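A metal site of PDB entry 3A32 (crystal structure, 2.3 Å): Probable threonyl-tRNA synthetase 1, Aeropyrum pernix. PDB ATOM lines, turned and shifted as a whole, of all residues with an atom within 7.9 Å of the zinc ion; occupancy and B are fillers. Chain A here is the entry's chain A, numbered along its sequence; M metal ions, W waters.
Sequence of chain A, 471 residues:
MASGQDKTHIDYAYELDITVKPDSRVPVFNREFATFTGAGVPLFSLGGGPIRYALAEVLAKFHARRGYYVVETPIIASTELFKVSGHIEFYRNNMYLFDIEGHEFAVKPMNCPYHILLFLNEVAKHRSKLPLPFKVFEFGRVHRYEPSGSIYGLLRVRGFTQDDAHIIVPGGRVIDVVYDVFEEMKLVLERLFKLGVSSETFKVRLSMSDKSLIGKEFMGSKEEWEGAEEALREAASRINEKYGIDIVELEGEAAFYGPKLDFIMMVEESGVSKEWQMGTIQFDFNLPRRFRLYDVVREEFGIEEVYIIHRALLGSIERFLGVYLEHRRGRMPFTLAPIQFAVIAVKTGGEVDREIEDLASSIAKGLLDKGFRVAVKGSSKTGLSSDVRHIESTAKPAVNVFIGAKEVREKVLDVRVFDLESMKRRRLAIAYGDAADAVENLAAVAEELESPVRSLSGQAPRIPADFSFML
A ring nitrogen (ND1) of His 115 sits at hydrogen-bond distance from a ring nitrogen (ND1) of His 166 (2.9 Å).
OD2 of Asp 284 sits at hydrogen-bond distance from NE2 of His 310, 2.6 Å away.
O of Gln 282 sits at hydrogen-bond distance from N of His 310 (2.7 Å).
Along chain A the residues within 4 Å of the zinc ion span positions 112 to 310.
The zinc ion is bound by a ring nitrogen (NE2) of His 166 (2.0 Å), water W1 (2.0 Å), a ring nitrogen (ND1) of His 310 (2.1 Å) and the side-chain sulfur of Cys 112 (2.3 Å).
The zinc ion has four donor atoms within binding distance.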
ATOM      1  N   MET A 110     -20.800   2.388 -13.273  1.00  0.00           N
ATOM      2  CA  MET A 110     -21.433   1.305 -12.531  1.00  0.00           C
ATOM      3  C   MET A 110     -20.950   1.328 -11.109  1.00  0.00           C
ATOM      4  O   MET A 110     -19.825   1.785 -10.857  1.00  0.00           O
ATOM      5  CB  MET A 110     -21.066  -0.039 -13.175  1.00  0.00           C
ATOM      6  CG  MET A 110     -19.565  -0.380 -13.229  1.00  0.00           C
ATOM      7  SD  MET A 110     -19.165  -1.663 -14.514  1.00  0.00           S
ATOM      8  CE  MET A 110     -20.832  -2.149 -15.059  1.00  0.00           C
ATOM      9  N   ASN A 111     -21.767   0.823 -10.173  1.00  0.00           N
ATOM     10  CA  ASN A 111     -21.413   0.847  -8.709  1.00  0.00           C
ATOM     11  C   ASN A 111     -20.673  -0.378  -8.251  1.00  0.00           C
ATOM     12  O   ASN A 111     -20.037  -0.355  -7.192  1.00  0.00           O
ATOM     13  CB  ASN A 111     -22.623   1.006  -7.813  1.00  0.00           C
ATOM     14  CG  ASN A 111     -23.523   2.137  -8.223  1.00  0.00           C
ATOM     15  OD1 ASN A 111     -24.694   1.945  -8.551  1.00  0.00           O
ATOM     16  ND2 ASN A 111     -22.997   3.330  -8.189  1.00  0.00           N
ATOM     17  N   CYS A 112     -20.744  -1.449  -9.049  1.00  0.00           N
ATOM     18  CA  CYS A 112     -20.161  -2.773  -8.712  1.00  0.00           C
ATOM     19  C   CYS A 112     -18.771  -2.835  -8.074  1.00  0.00           C
ATOM     20  O   CYS A 112     -18.635  -3.516  -7.048  1.00  0.00           O
ATOM     21  CB  CYS A 112     -20.191  -3.739  -9.948  1.00  0.00           C
ATOM     22  SG  CYS A 112     -21.386  -3.292 -11.255  1.00  0.00           S
ATOM     23  N   PRO A 113     -17.729  -2.267  -8.728  1.00  0.00           N
ATOM     24  CA  PRO A 113     -16.373  -2.275  -8.169  1.00  0.00           C
ATOM     25  C   PRO A 113     -16.285  -1.565  -6.815  1.00  0.00           C
ATOM     26  O   PRO A 113     -15.560  -2.042  -5.928  1.00  0.00           O
ATOM     27  CB  PRO A 113     -15.541  -1.523  -9.240  1.00  0.00           C
ATOM     28  CG  PRO A 113     -16.333  -1.715 -10.548  1.00  0.00           C
ATOM     29  CD  PRO A 113     -17.768  -1.715 -10.098  1.00  0.00           C
ATOM     30  N   HIS A 115     -18.816  -1.359  -4.599  1.00  0.00           N
ATOM     31  CA  HIS A 115     -19.513  -2.276  -3.643  1.00  0.00           C
ATOM     32  C   HIS A 115     -18.635  -3.447  -3.265  1.00  0.00           C
ATOM     33  O   HIS A 115     -18.694  -3.878  -2.139  1.00  0.00           O
ATOM     34  CB  HIS A 115     -20.849  -2.789  -4.233  1.00  0.00           C
ATOM     35  CG  HIS A 115     -21.888  -1.711  -4.335  1.00  0.00           C
ATOM     36  ND1 HIS A 115     -23.207  -1.973  -4.655  1.00  0.00           N
ATOM     37  CD2 HIS A 115     -21.801  -0.375  -4.125  1.00  0.00           C
ATOM     38  CE1 HIS A 115     -23.884  -0.844  -4.625  1.00  0.00           C
ATOM     39  NE2 HIS A 115     -23.064   0.137  -4.312  1.00  0.00           N
ATOM     40  N   ILE A 116     -17.814  -3.931  -4.218  1.00  0.00           N
ATOM     41  CA  ILE A 116     -16.814  -4.988  -3.937  1.00  0.00           C
ATOM     42  C   ILE A 116     -15.661  -4.512  -3.066  1.00  0.00           C
ATOM     43  O   ILE A 116     -15.234  -5.235  -2.200  1.00  0.00           O
ATOM     44  CB  ILE A 116     -16.248  -5.637  -5.209  1.00  0.00           C
ATOM     45  CG1 ILE A 116     -17.366  -6.352  -5.952  1.00  0.00           C
ATOM     46  CG2 ILE A 116     -15.097  -6.652  -4.853  1.00  0.00           C
ATOM     47  CD1 ILE A 116     -17.008  -6.494  -7.399  1.00  0.00           C
ATOM     48  N   ARG A 144     -22.904   7.398 -18.463  1.00  0.00           N
ATOM     49  CA  ARG A 144     -22.443   6.550 -19.568  1.00  0.00           C
ATOM     50  C   ARG A 144     -22.528   7.361 -20.845  1.00  0.00           C
ATOM     51  O   ARG A 144     -23.418   8.197 -20.990  1.00  0.00           O
ATOM     52  CB  ARG A 144     -23.327   5.309 -19.655  1.00  0.00           C
ATOM     53  CG  ARG A 144     -23.132   4.419 -18.471  1.00  0.00           C
ATOM     54  CD  ARG A 144     -24.014   3.226 -18.533  1.00  0.00           C
ATOM     55  NE  ARG A 144     -23.845   2.430 -17.312  1.00  0.00           N
ATOM     56  CZ  ARG A 144     -24.539   1.313 -17.055  1.00  0.00           C
ATOM     57  NH1 ARG A 144     -25.405   0.873 -17.944  1.00  0.00           N
ATOM     58  NH2 ARG A 144     -24.378   0.644 -15.914  1.00  0.00           N
ATOM     59  N   GLN A 162     -30.031   3.913 -10.506  1.00  0.00           N
ATOM     60  CA  GLN A 162     -30.386   2.470 -10.449  1.00  0.00           C
ATOM     61  C   GLN A 162     -30.683   2.162  -8.978  1.00  0.00           C
ATOM     62  O   GLN A 162     -30.041   2.738  -8.111  1.00  0.00           O
ATOM     63  CB  GLN A 162     -29.170   1.615 -10.796  1.00  0.00           C
ATOM     64  CG  GLN A 162     -28.697   1.697 -12.209  1.00  0.00           C
ATOM     65  CD  GLN A 162     -27.284   1.216 -12.396  1.00  0.00           C
ATOM     66  OE1 GLN A 162     -26.406   1.430 -11.569  1.00  0.00           O
ATOM     67  NE2 GLN A 162     -27.052   0.555 -13.519  1.00  0.00           N
ATOM     68  N   ASP A 164     -29.627  -0.369  -7.287  1.00  0.00           N
ATOM     69  CA  ASP A 164     -28.579  -1.313  -7.535  1.00  0.00           C
ATOM     70  C   ASP A 164     -28.216  -2.070  -6.254  1.00  0.00           C
ATOM     71  O   ASP A 164     -28.106  -1.464  -5.185  1.00  0.00           O
ATOM     72  CB  ASP A 164     -27.360  -0.515  -8.034  1.00  0.00           C
ATOM     73  CG  ASP A 164     -26.337  -1.389  -8.766  1.00  0.00           C
ATOM     74  OD1 ASP A 164     -26.707  -2.482  -9.253  1.00  0.00           O
ATOM     75  OD2 ASP A 164     -25.164  -0.945  -8.870  1.00  0.00           O
ATOM     76  N   ALA A 165     -27.937  -3.382  -6.363  1.00  0.00           N
ATOM     77  CA  ALA A 165     -27.426  -4.110  -5.215  1.00  0.00           C
ATOM     78  C   ALA A 165     -26.509  -5.189  -5.709  1.00  0.00           C
ATOM     79  O   ALA A 165     -26.584  -5.600  -6.874  1.00  0.00           O
ATOM     80  CB  ALA A 165     -28.583  -4.686  -4.391  1.00  0.00           C
ATOM     81  N   HIS A 166     -25.605  -5.613  -4.832  1.00  0.00           N
ATOM     82  CA  HIS A 166     -24.724  -6.709  -5.079  1.00  0.00           C
ATOM     83  C   HIS A 166     -24.807  -7.710  -3.940  1.00  0.00           C
ATOM     84  O   HIS A 166     -24.905  -7.341  -2.757  1.00  0.00           O
ATOM     85  CB  HIS A 166     -23.293  -6.208  -5.356  1.00  0.00           C
ATOM     86  CG  HIS A 166     -23.227  -5.410  -6.628  1.00  0.00           C
ATOM     87  ND1 HIS A 166     -23.452  -4.060  -6.657  1.00  0.00           N
ATOM     88  CD2 HIS A 166     -23.110  -5.808  -7.912  1.00  0.00           C
ATOM     89  CE1 HIS A 166     -23.420  -3.631  -7.911  1.00  0.00           C
ATOM     90  NE2 HIS A 166     -23.211  -4.669  -8.692  1.00  0.00           N
ATOM     91  N   TYR A 257     -20.228 -13.275 -18.992  1.00  0.00           N
ATOM     92  CA  TYR A 257     -19.787 -13.497 -17.592  1.00  0.00           C
ATOM     93  C   TYR A 257     -20.818 -14.117 -16.680  1.00  0.00           C
ATOM     94  O   TYR A 257     -20.563 -14.204 -15.467  1.00  0.00           O
ATOM     95  CB  TYR A 257     -19.309 -12.186 -16.909  1.00  0.00           C
ATOM     96  CG  TYR A 257     -20.297 -11.058 -17.063  1.00  0.00           C
ATOM     97  CD1 TYR A 257     -21.298 -10.807 -16.124  1.00  0.00           C
ATOM     98  CD2 TYR A 257     -20.275 -10.265 -18.221  1.00  0.00           C
ATOM     99  CE1 TYR A 257     -22.226  -9.758 -16.321  1.00  0.00           C
ATOM    100  CE2 TYR A 257     -21.187  -9.233 -18.433  1.00  0.00           C
ATOM    101  CZ  TYR A 257     -22.145  -8.979 -17.466  1.00  0.00           C
ATOM    102  OH  TYR A 257     -23.021  -7.939 -17.727  1.00  0.00           O
ATOM    103  N   GLN A 282     -28.394 -10.841 -12.255  1.00  0.00           N
ATOM    104  CA  GLN A 282     -27.237 -11.165 -13.081  1.00  0.00           C
ATOM    105  C   GLN A 282     -26.017 -11.715 -12.286  1.00  0.00           C
ATOM    106  O   GLN A 282     -25.376 -10.998 -11.521  1.00  0.00           O
ATOM    107  CB  GLN A 282     -26.839  -9.905 -13.864  1.00  0.00           C
ATOM    108  CG  GLN A 282     -25.533 -10.043 -14.630  1.00  0.00           C
ATOM    109  CD  GLN A 282     -25.744 -10.803 -15.933  1.00  0.00           C
ATOM    110  OE1 GLN A 282     -26.460 -10.345 -16.814  1.00  0.00           O
ATOM    111  NE2 GLN A 282     -25.082 -11.976 -16.059  1.00  0.00           N
ATOM    112  N   ASP A 284     -22.136 -13.328 -12.207  1.00  0.00           N
ATOM    113  CA  ASP A 284     -20.902 -12.775 -12.657  1.00  0.00           C
ATOM    114  C   ASP A 284     -19.790 -13.713 -12.209  1.00  0.00           C
ATOM    115  O   ASP A 284     -19.619 -13.981 -11.005  1.00  0.00           O
ATOM    116  CB  ASP A 284     -20.749 -11.361 -12.092  1.00  0.00           C
ATOM    117  CG  ASP A 284     -19.699 -10.552 -12.831  1.00  0.00           C
ATOM    118  OD1 ASP A 284     -18.621 -11.142 -13.161  1.00  0.00           O
ATOM    119  OD2 ASP A 284     -19.949  -9.339 -13.057  1.00  0.00           O
ATOM    120  N   LEU A 287     -16.062 -10.950 -12.083  1.00  0.00           N
ATOM    121  CA  LEU A 287     -15.715 -10.133 -10.904  1.00  0.00           C
ATOM    122  C   LEU A 287     -15.047 -10.920  -9.782  1.00  0.00           C
ATOM    123  O   LEU A 287     -14.107 -10.425  -9.192  1.00  0.00           O
ATOM    124  CB  LEU A 287     -16.943  -9.371 -10.330  1.00  0.00           C
ATOM    125  CG  LEU A 287     -17.484  -8.076 -10.960  1.00  0.00           C
ATOM    126  CD1 LEU A 287     -18.743  -7.492 -10.240  1.00  0.00           C
ATOM    127  CD2 LEU A 287     -16.390  -6.961 -11.218  1.00  0.00           C
ATOM    128  N   ILE A 308     -21.612 -14.412  -7.136  1.00  0.00           N
ATOM    129  CA  ILE A 308     -21.650 -12.960  -7.142  1.00  0.00           C
ATOM    130  C   ILE A 308     -22.827 -12.516  -8.046  1.00  0.00           C
ATOM    131  O   ILE A 308     -22.957 -12.943  -9.226  1.00  0.00           O
ATOM    132  CB  ILE A 308     -20.314 -12.363  -7.624  1.00  0.00           C
ATOM    133  CG1 ILE A 308     -19.266 -12.334  -6.522  1.00  0.00           C
ATOM    134  CG2 ILE A 308     -20.513 -10.906  -8.020  1.00  0.00           C
ATOM    135  CD1 ILE A 308     -18.769 -13.680  -5.946  1.00  0.00           C
ATOM    136  N   ILE A 309     -23.694 -11.680  -7.480  1.00  0.00           N
ATOM    137  CA  ILE A 309     -24.875 -11.283  -8.196  1.00  0.00           C
ATOM    138  C   ILE A 309     -24.987  -9.747  -8.230  1.00  0.00           C
ATOM    139  O   ILE A 309     -24.783  -9.083  -7.228  1.00  0.00           O
ATOM    140  CB  ILE A 309     -26.155 -11.938  -7.571  1.00  0.00           C
ATOM    141  CG1 ILE A 309     -26.129 -13.455  -7.762  1.00  0.00           C
ATOM    142  CG2 ILE A 309     -27.441 -11.322  -8.161  1.00  0.00           C
ATOM    143  CD1 ILE A 309     -27.182 -14.236  -6.992  1.00  0.00           C
ATOM    144  N   HIS A 310     -25.279  -9.232  -9.419  1.00  0.00           N
ATOM    145  CA  HIS A 310     -25.774  -7.877  -9.632  1.00  0.00           C
ATOM    146  C   HIS A 310     -27.297  -8.004  -9.698  1.00  0.00           C
ATOM    147  O   HIS A 310     -27.794  -8.915 -10.360  1.00  0.00           O
ATOM    148  CB  HIS A 310     -25.408  -7.376 -11.022  1.00  0.00           C
ATOM    149  CG  HIS A 310     -23.948  -7.472 -11.381  1.00  0.00           C
ATOM    150  ND1 HIS A 310     -23.110  -6.383 -11.342  1.00  0.00           N
ATOM    151  CD2 HIS A 310     -23.206  -8.514 -11.843  1.00  0.00           C
ATOM    152  CE1 HIS A 310     -21.908  -6.748 -11.760  1.00  0.00           C
ATOM    153  NE2 HIS A 310     -21.945  -8.028 -12.079  1.00  0.00           N
ATOM    154  N   ARG A 311     -28.052  -7.099  -9.064  1.00  0.00           N
ATOM    155  CA  ARG A 311     -29.512  -7.141  -9.207  1.00  0.00           C
ATOM    156  C   ARG A 311     -30.134  -5.761  -9.084  1.00  0.00           C
ATOM    157  O   ARG A 311     -29.674  -4.966  -8.297  1.00  0.00           O
ATOM    158  CB  ARG A 311     -30.139  -8.115  -8.192  1.00  0.00           C
ATOM    159  CG  ARG A 311     -29.776  -7.931  -6.700  1.00  0.00           C
ATOM    160  CD  ARG A 311     -30.902  -7.271  -5.873  1.00  0.00           C
ATOM    161  NE  ARG A 311     -31.094  -5.828  -6.093  1.00  0.00           N
ATOM    162  CZ  ARG A 311     -32.020  -5.096  -5.466  1.00  0.00           C
ATOM    163  NH1 ARG A 311     -32.852  -5.659  -4.571  1.00  0.00           N
ATOM    164  NH2 ARG A 311     -32.131  -3.792  -5.720  1.00  0.00           N
HETATM  165 ZN    ZN M   1     -23.270  -4.440 -10.666  1.00  0.00          ZN
HETATM  166  O   HOH W   1     -25.152  -3.747 -10.893  1.00  0.00           O
